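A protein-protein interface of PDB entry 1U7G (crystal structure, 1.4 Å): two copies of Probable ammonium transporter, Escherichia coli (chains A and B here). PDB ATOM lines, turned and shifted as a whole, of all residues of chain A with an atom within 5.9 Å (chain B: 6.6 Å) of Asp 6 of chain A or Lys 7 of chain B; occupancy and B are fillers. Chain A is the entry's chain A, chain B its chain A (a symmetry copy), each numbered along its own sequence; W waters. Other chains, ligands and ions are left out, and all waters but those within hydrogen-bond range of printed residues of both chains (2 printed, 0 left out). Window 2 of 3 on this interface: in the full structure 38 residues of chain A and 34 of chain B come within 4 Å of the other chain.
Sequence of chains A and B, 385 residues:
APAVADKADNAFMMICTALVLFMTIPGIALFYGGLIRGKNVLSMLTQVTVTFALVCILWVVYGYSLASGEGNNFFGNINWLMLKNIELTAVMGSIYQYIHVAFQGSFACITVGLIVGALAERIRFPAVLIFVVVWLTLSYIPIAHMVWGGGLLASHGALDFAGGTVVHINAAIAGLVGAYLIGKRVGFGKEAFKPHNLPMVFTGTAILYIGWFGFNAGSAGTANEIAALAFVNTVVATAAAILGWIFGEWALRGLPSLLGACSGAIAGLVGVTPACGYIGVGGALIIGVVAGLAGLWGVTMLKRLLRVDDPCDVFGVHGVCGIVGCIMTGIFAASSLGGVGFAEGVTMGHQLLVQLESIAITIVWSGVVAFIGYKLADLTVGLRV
The side-chain carboxylate of Asp 6 of chain A is in hydrogen-bond range of the backbone NH of Asp 9 of chain A, 3.1 Å away. N of Asp 6 of chain A sits at hydrogen-bond distance from O of Ser 94 of chain A (2.8 Å). The side-chain carboxylate (OD2) of Asp 9 of chain A is in hydrogen-bond range of the side-chain hydroxyl (OG) of Ser 94 of chain A, 2.7 Å away. OD1 of Asp 9 of chain A lies within hydrogen-bond range of OG1 of Thr 222 of chain A, at 2.7 Å. The backbone NH of Ala 223 of chain A lies within hydrogen-bond range of the side-chain carboxylate of Asp 9 of chain A (2.8 Å). The side-chain carboxylate (OD2) of Asp 6 of chain B is in hydrogen-bond range of the backbone NH (N) of Ala 8 of chain B (2.8 Å).
Of chain B, only Lys 7 (2.9 Å) comes within 4 Å of Asp 6 of chain A. Lys 7 of chain B touches five residues of chain A. Printed residues of chain A within 4 Å of Ala 8 of chain B: Ala 8 (3.2 Å). Of the printed residues of chain A, Met 14 of chain B touches Ala 223. Of the printed residues of chain A, Ala 11 of chain B touches Ala 8 and Ala 223. Printed residues of chain B within 4 Å of Ala 8 of chain A: Lys 7, Ala 8 and Ala 11. Printed residues of chain A within 4 Å of Asn 10 of chain B: Ala 223 (2.9 Å). Asp 6 of chain B touches none of the printed residues of chain A. The nearest residue of chain B that does not touch Asp 6 of chain A is Ala 8 of chain B (5.7 Å). The nearest residue of chain A that does not touch Lys 7 of chain B is Ser 94 of chain A (4.5 Å). The nearest printed residue of chain A that does not touch Ala 8 of chain B is Asp 6 of chain A (5.7 Å).
Water W1 lies within hydrogen-bond range of the side-chain hydroxyl of Thr 222 of chain A and the side-chain amino group of Lys 7 of chain B. Water W2 lies within hydrogen-bond range of the side-chain amino group (NZ) of Lys 7 of chain B (2.8 Å) and the side-chain carboxylate (OD1) of Asp 6 of chain A (2.9 Å).
Asp 6 of chain A touches Lys 7 of chain B, but with the chains exchanged Lys 7 of chain A does not touch Asp 6 of chain B (8.5 Å). Ala 8 of chain A touches Lys 7 of chain B, but with the chains exchanged Lys 7 of chain A does not touch Ala 8 of chain B (6.4 Å). Ala 8 of chain A touches its own counterpart, Ala 8 of chain B. Ala 8 of chain A touches Ala 11 of chain B, but with the chains exchanged Ala 11 of chain A does not touch Ala 8 of chain B (6.7 Å). Of the 11 pairs that touch across the chains among the printed residues, 1 has its exchanged pair printed and touching as well.
Of the 11 printed residues of chain B, 6 touch a printed residue of chain A. Hydrophobic or aromatic side chains of chain B within 4 Å of the printed part of chain A: Ala 11, Met 14 and Tyr 96. Of the 13 printed residues of chain A, 6 touch a printed residue of chain B. Printed residues of chain A that touch a printed residue of chain B: Asp 6, Ala 8, Asp 9, Thr 222, Ala 223 and Asn 224. Among the printed residues, 11 pairs touch across the chains. Among the printed residues, Asp or Glu carboxylates within 4 Å of a Lys or Arg side-chain nitrogen of the other chain: Asp 6 of chain A with Lys 7 of chain B and Asp 9 of chain A with Lys 7 of chain B.
Among the printed residues, merely in contact across the chains: Ala 8 of chain A with Lys 7 of chain B, Ala 8 of chain A with Ala 8 of chain B, Ala 8 of chain A with Ala 11 of chain B, Thr 222 of chain A with Lys 7 of chain B, Ala 223 of chain A with Lys 7 of chain B, Ala 223 of chain A with Ala 11 of chain B, Ala 223 of chain A with Met 14 of chain B and Asn 224 of chain A with Tyr 96 of chain B.
The side-chain amino group of Lys 7 of chain B lies within salt-bridge range of the side-chain carboxylate of Asp 6 of chain A (3.1 Å). The side-chain amino group of Lys 7 of chain B lies within salt-bridge range of the side-chain carboxylate of Asp 9 of chain A, at 2.6 Å. The side-chain amide nitrogen of Asn 10 of chain B lies within hydrogen-bond range of the backbone carbonyl oxygen of Ala 223 of chain A (2.9 Å).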
ATOM      1  N   VAL A   4     -17.494  -1.403  -7.456  1.00  0.00           N
ATOM      2  CA  VAL A   4     -17.951  -1.130  -6.080  1.00  0.00           C
ATOM      3  C   VAL A   4     -17.602  -2.299  -5.181  1.00  0.00           C
ATOM      4  O   VAL A   4     -17.556  -3.468  -5.545  1.00  0.00           O
ATOM      5  CB  VAL A   4     -19.444  -0.757  -6.081  1.00  0.00           C
ATOM      6  CG1 VAL A   4     -20.147  -0.955  -4.751  1.00  0.00           C
ATOM      7  CG2 VAL A   4     -19.585   0.724  -6.437  1.00  0.00           C
ATOM      8  N   ALA A   5     -17.265  -1.984  -3.933  1.00  0.00           N
ATOM      9  CA  ALA A   5     -16.812  -3.047  -3.048  1.00  0.00           C
ATOM     10  C   ALA A   5     -17.985  -3.861  -2.543  1.00  0.00           C
ATOM     11  O   ALA A   5     -19.076  -3.374  -2.225  1.00  0.00           O
ATOM     12  CB  ALA A   5     -16.055  -2.436  -1.871  1.00  0.00           C
ATOM     13  N   ASP A   6     -17.747  -5.153  -2.431  1.00  0.00           N
ATOM     14  CA  ASP A   6     -18.699  -6.027  -1.791  1.00  0.00           C
ATOM     15  C   ASP A   6     -18.299  -6.211  -0.328  1.00  0.00           C
ATOM     16  O   ASP A   6     -17.157  -6.655  -0.130  1.00  0.00           O
ATOM     17  CB  ASP A   6     -18.684  -7.356  -2.538  1.00  0.00           C
ATOM     18  CG  ASP A   6     -19.657  -8.358  -1.970  1.00  0.00           C
ATOM     19  OD1 ASP A   6     -20.511  -8.841  -2.724  1.00  0.00           O
ATOM     20  OD2 ASP A   6     -19.614  -8.714  -0.805  1.00  0.00           O
ATOM     21  N   LYS A   7     -19.188  -5.808   0.570  1.00  0.00           N
ATOM     22  CA  LYS A   7     -18.765  -5.859   1.972  1.00  0.00           C
ATOM     23  C   LYS A   7     -18.486  -7.277   2.425  1.00  0.00           C
ATOM     24  O   LYS A   7     -17.655  -7.462   3.309  1.00  0.00           O
ATOM     25  CB  LYS A   7     -19.842  -5.197   2.827  1.00  0.00           C
ATOM     26  CG  LYS A   7     -19.838  -3.667   2.668  1.00  0.00           C
ATOM     27  CD  LYS A   7     -20.533  -2.969   3.817  1.00  0.00           C
ATOM     28  CE  LYS A   7     -21.936  -3.377   4.066  1.00  0.00           C
ATOM     29  NZ  LYS A   7     -22.706  -2.491   5.008  1.00  0.00           N
ATOM     30  N   ALA A   8     -19.168  -8.263   1.870  1.00  0.00           N
ATOM     31  CA  ALA A   8     -18.868  -9.648   2.227  1.00  0.00           C
ATOM     32  C   ALA A   8     -17.416  -9.973   1.868  1.00  0.00           C
ATOM     33  O   ALA A   8     -16.714 -10.614   2.638  1.00  0.00           O
ATOM     34  CB  ALA A   8     -19.793 -10.655   1.511  1.00  0.00           C
ATOM     35  N   ASP A   9     -16.975  -9.547   0.690  1.00  0.00           N
ATOM     36  CA  ASP A   9     -15.616  -9.791   0.292  1.00  0.00           C
ATOM     37  C   ASP A   9     -14.665  -8.957   1.126  1.00  0.00           C
ATOM     38  O   ASP A   9     -13.606  -9.446   1.514  1.00  0.00           O
ATOM     39  CB  ASP A   9     -15.422  -9.470  -1.196  1.00  0.00           C
ATOM     40  CG  ASP A   9     -16.216 -10.442  -2.055  1.00  0.00           C
ATOM     41  OD1 ASP A   9     -16.521 -11.564  -1.633  1.00  0.00           O
ATOM     42  OD2 ASP A   9     -16.505 -10.042  -3.200  1.00  0.00           O
ATOM     43  N   ASN A  10     -15.063  -7.703   1.395  1.00  0.00           N
ATOM     44  CA  ASN A  10     -14.207  -6.924   2.301  1.00  0.00           C
ATOM     45  C   ASN A  10     -14.005  -7.666   3.637  1.00  0.00           C
ATOM     46  O   ASN A  10     -12.871  -7.717   4.130  1.00  0.00           O
ATOM     47  CB  ASN A  10     -14.820  -5.578   2.642  1.00  0.00           C
ATOM     48  CG  ASN A  10     -14.842  -4.607   1.480  1.00  0.00           C
ATOM     49  OD1 ASN A  10     -14.083  -4.680   0.517  1.00  0.00           O
ATOM     50  ND2 ASN A  10     -15.788  -3.668   1.642  1.00  0.00           N
ATOM     51  N   ALA A  11     -15.084  -8.134   4.210  1.00  0.00           N
ATOM     52  CA  ALA A  11     -15.032  -8.810   5.490  1.00  0.00           C
ATOM     53  C   ALA A  11     -14.143 -10.049   5.393  1.00  0.00           C
ATOM     54  O   ALA A  11     -13.219 -10.254   6.184  1.00  0.00           O
ATOM     55  CB  ALA A  11     -16.429  -9.243   5.898  1.00  0.00           C
ATOM     56  N   SER A  94     -13.181  -6.906  -5.955  1.00  0.00           N
ATOM     57  CA  SER A  94     -14.458  -6.571  -5.348  1.00  0.00           C
ATOM     58  C   SER A  94     -14.259  -6.111  -3.901  1.00  0.00           C
ATOM     59  O   SER A  94     -15.203  -6.160  -3.140  1.00  0.00           O
ATOM     60  CB  SER A  94     -15.355  -7.807  -5.384  1.00  0.00           C
ATOM     61  OG  SER A  94     -14.683  -8.912  -4.790  1.00  0.00           O
ATOM     62  N   ILE A  95     -13.038  -5.701  -3.601  1.00  0.00           N
ATOM     63  CA  ILE A  95     -12.799  -5.204  -2.255  1.00  0.00           C
ATOM     64  C   ILE A  95     -12.116  -3.835  -2.310  1.00  0.00           C
ATOM     65  O   ILE A  95     -11.558  -3.439  -3.327  1.00  0.00           O
ATOM     66  CB  ILE A  95     -11.932  -6.186  -1.451  1.00  0.00           C
ATOM     67  CG1 ILE A  95     -10.547  -6.297  -2.084  1.00  0.00           C
ATOM     68  CG2 ILE A  95     -12.631  -7.543  -1.278  1.00  0.00           C
ATOM     69  CD1 ILE A  95      -9.648  -7.291  -1.348  1.00  0.00           C
ATOM     70  N   THR A 222     -12.373 -13.041  -2.899  1.00  0.00           N
ATOM     71  CA  THR A 222     -13.820 -12.917  -2.746  1.00  0.00           C
ATOM     72  C   THR A 222     -14.279 -14.186  -2.051  1.00  0.00           C
ATOM     73  O   THR A 222     -13.631 -15.234  -2.218  1.00  0.00           O
ATOM     74  CB  THR A 222     -14.512 -12.741  -4.128  1.00  0.00           C
ATOM     75  OG1 THR A 222     -15.900 -12.967  -3.901  1.00  0.00           O
ATOM     76  CG2 THR A 222     -13.938 -13.773  -5.107  1.00  0.00           C
ATOM     77  N   ALA A 223     -15.350 -14.132  -1.300  1.00  0.00           N
ATOM     78  CA  ALA A 223     -15.880 -15.296  -0.622  1.00  0.00           C
ATOM     79  C   ALA A 223     -16.837 -16.006  -1.585  1.00  0.00           C
ATOM     80  O   ALA A 223     -18.053 -15.991  -1.371  1.00  0.00           O
ATOM     81  CB  ALA A 223     -16.567 -14.878   0.650  1.00  0.00           C
ATOM     82  N   ASN A 224     -16.222 -16.591  -2.616  1.00  0.00           N
ATOM     83  CA  ASN A 224     -17.064 -17.268  -3.612  1.00  0.00           C
ATOM     84  C   ASN A 224     -16.764 -18.761  -3.630  1.00  0.00           C
ATOM     85  O   ASN A 224     -16.173 -19.338  -2.737  1.00  0.00           O
ATOM     86  CB  ASN A 224     -16.822 -16.567  -4.951  1.00  0.00           C
ATOM     87  CG  ASN A 224     -15.474 -16.796  -5.581  1.00  0.00           C
ATOM     88  OD1 ASN A 224     -15.172 -16.460  -6.768  1.00  0.00           O
ATOM     89  ND2 ASN A 224     -14.533 -17.343  -4.879  1.00  0.00           N
ATOM     90  N   ALA B   5     -25.842 -18.443  -3.535  1.00  0.00           N
ATOM     91  CA  ALA B   5     -25.050 -18.266  -2.326  1.00  0.00           C
ATOM     92  C   ALA B   5     -24.987 -16.804  -1.934  1.00  0.00           C
ATOM     93  O   ALA B   5     -24.877 -15.877  -2.744  1.00  0.00           O
ATOM     94  CB  ALA B   5     -23.642 -18.805  -2.561  1.00  0.00           C
ATOM     95  N   ASP B   6     -25.024 -16.583  -0.635  1.00  0.00           N
ATOM     96  CA  ASP B   6     -24.787 -15.265  -0.102  1.00  0.00           C
ATOM     97  C   ASP B   6     -23.317 -15.150   0.304  1.00  0.00           C
ATOM     98  O   ASP B   6     -22.915 -15.988   1.125  1.00  0.00           O
ATOM     99  CB  ASP B   6     -25.706 -15.077   1.099  1.00  0.00           C
ATOM    100  CG  ASP B   6     -25.562 -13.719   1.739  1.00  0.00           C
ATOM    101  OD1 ASP B   6     -26.571 -13.010   1.850  1.00  0.00           O
ATOM    102  OD2 ASP B   6     -24.494 -13.312   2.164  1.00  0.00           O
ATOM    103  N   LYS B   7     -22.616 -14.214  -0.322  1.00  0.00           N
ATOM    104  CA  LYS B   7     -21.179 -14.180  -0.038  1.00  0.00           C
ATOM    105  C   LYS B   7     -20.901 -13.859   1.415  1.00  0.00           C
ATOM    106  O   LYS B   7     -19.878 -14.299   1.932  1.00  0.00           O
ATOM    107  CB  LYS B   7     -20.525 -13.166  -0.972  1.00  0.00           C
ATOM    108  CG  LYS B   7     -20.435 -13.694  -2.415  1.00  0.00           C
ATOM    109  CD  LYS B   7     -19.399 -12.955  -3.234  1.00  0.00           C
ATOM    110  CE  LYS B   7     -19.574 -11.484  -3.317  1.00  0.00           C
ATOM    111  NZ  LYS B   7     -18.725 -10.794  -4.352  1.00  0.00           N
ATOM    112  N   ALA B   8     -21.754 -13.092   2.068  1.00  0.00           N
ATOM    113  CA  ALA B   8     -21.558 -12.827   3.492  1.00  0.00           C
ATOM    114  C   ALA B   8     -21.591 -14.143   4.273  1.00  0.00           C
ATOM    115  O   ALA B   8     -20.782 -14.358   5.165  1.00  0.00           O
ATOM    116  CB  ALA B   8     -22.630 -11.879   4.071  1.00  0.00           C
ATOM    117  N   ASP B   9     -22.542 -15.013   3.949  1.00  0.00           N
ATOM    118  CA  ASP B   9     -22.623 -16.281   4.620  1.00  0.00           C
ATOM    119  C   ASP B   9     -21.459 -17.165   4.221  1.00  0.00           C
ATOM    120  O   ASP B   9     -20.902 -17.859   5.068  1.00  0.00           O
ATOM    121  CB  ASP B   9     -23.946 -16.984   4.290  1.00  0.00           C
ATOM    122  CG  ASP B   9     -25.117 -16.206   4.871  1.00  0.00           C
ATOM    123  OD1 ASP B   9     -24.966 -15.459   5.844  1.00  0.00           O
ATOM    124  OD2 ASP B   9     -26.221 -16.399   4.322  1.00  0.00           O
ATOM    125  N   ASN B  10     -21.103 -17.120   2.926  1.00  0.00           N
ATOM    126  CA  ASN B  10     -19.902 -17.879   2.551  1.00  0.00           C
ATOM    127  C   ASN B  10     -18.692 -17.447   3.402  1.00  0.00           C
ATOM    128  O   ASN B  10     -17.947 -18.317   3.871  1.00  0.00           O
ATOM    129  CB  ASN B  10     -19.516 -17.648   1.101  1.00  0.00           C
ATOM    130  CG  ASN B  10     -20.480 -18.265   0.108  1.00  0.00           C
ATOM    131  OD1 ASN B  10     -21.222 -19.204   0.375  1.00  0.00           O
ATOM    132  ND2 ASN B  10     -20.411 -17.656  -1.087  1.00  0.00           N
ATOM    133  N   ALA B  11     -18.485 -16.159   3.505  1.00  0.00           N
ATOM    134  CA  ALA B  11     -17.355 -15.628   4.240  1.00  0.00           C
ATOM    135  C   ALA B  11     -17.422 -16.074   5.700  1.00  0.00           C
ATOM    136  O   ALA B  11     -16.469 -16.618   6.261  1.00  0.00           O
ATOM    137  CB  ALA B  11     -17.379 -14.111   4.191  1.00  0.00           C
ATOM    138  N   PHE B  12     -18.597 -15.808   6.262  1.00  0.00           N
ATOM    139  CA  PHE B  12     -18.823 -16.219   7.646  1.00  0.00           C
ATOM    140  C   PHE B  12     -18.478 -17.675   7.870  1.00  0.00           C
ATOM    141  O   PHE B  12     -17.813 -18.090   8.809  1.00  0.00           O
ATOM    142  CB  PHE B  12     -20.285 -15.946   8.054  1.00  0.00           C
ATOM    143  CG  PHE B  12     -20.560 -16.218   9.514  1.00  0.00           C
ATOM    144  CD1 PHE B  12     -19.812 -15.572  10.474  1.00  0.00           C
ATOM    145  CD2 PHE B  12     -21.558 -17.087   9.847  1.00  0.00           C
ATOM    146  CE1 PHE B  12     -20.128 -15.856  11.818  1.00  0.00           C
ATOM    147  CE2 PHE B  12     -21.897 -17.393  11.159  1.00  0.00           C
ATOM    148  CZ  PHE B  12     -21.148 -16.738  12.139  1.00  0.00           C
ATOM    149  N   MET B  14     -16.834 -19.904   5.993  1.00  0.00           N
ATOM    150  CA  MET B  14     -15.441 -20.345   5.823  1.00  0.00           C
ATOM    151  C   MET B  14     -14.641 -19.949   7.052  1.00  0.00           C
ATOM    152  O   MET B  14     -13.826 -20.758   7.526  1.00  0.00           O
ATOM    153  CB  MET B  14     -14.805 -19.725   4.583  1.00  0.00           C
ATOM    154  CG  MET B  14     -15.235 -20.505   3.321  1.00  0.00           C
ATOM    155  SD  MET B  14     -14.415 -19.930   1.759  1.00  0.00           S
ATOM    156  CE  MET B  14     -15.499 -18.435   1.468  1.00  0.00           C
ATOM    157  N   SER B  94     -27.536 -21.179   2.350  1.00  0.00           N
ATOM    158  CA  SER B  94     -27.220 -19.954   1.636  1.00  0.00           C
ATOM    159  C   SER B  94     -25.715 -19.863   1.368  1.00  0.00           C
ATOM    160  O   SER B  94     -25.230 -18.775   1.138  1.00  0.00           O
ATOM    161  CB  SER B  94     -27.671 -18.765   2.483  1.00  0.00           C
ATOM    162  OG  SER B  94     -27.110 -18.857   3.788  1.00  0.00           O
ATOM    163  N   TYR B  96     -22.115 -21.865  -0.529  1.00  0.00           N
ATOM    164  CA  TYR B  96     -21.683 -22.958  -1.410  1.00  0.00           C
ATOM    165  C   TYR B  96     -21.599 -24.263  -0.633  1.00  0.00           C
ATOM    166  O   TYR B  96     -21.108 -24.306   0.504  1.00  0.00           O
ATOM    167  CB  TYR B  96     -20.338 -22.682  -2.116  1.00  0.00           C
ATOM    168  CG  TYR B  96     -20.624 -21.574  -3.129  1.00  0.00           C
ATOM    169  CD1 TYR B  96     -21.507 -21.840  -4.182  1.00  0.00           C
ATOM    170  CD2 TYR B  96     -20.030 -20.332  -2.986  1.00  0.00           C
ATOM    171  CE1 TYR B  96     -21.736 -20.783  -5.081  1.00  0.00           C
ATOM    172  CE2 TYR B  96     -20.271 -19.291  -3.877  1.00  0.00           C
ATOM    173  CZ  TYR B  96     -21.143 -19.560  -4.932  1.00  0.00           C
ATOM    174  OH  TYR B  96     -21.395 -18.540  -5.818  1.00  0.00           O
HETATM  175  O   HOH W   1     -17.482 -12.781  -6.031  1.00  0.00           O
HETATM  176  O   HOH W   2     -19.932  -8.646  -5.609  1.00  0.00           O
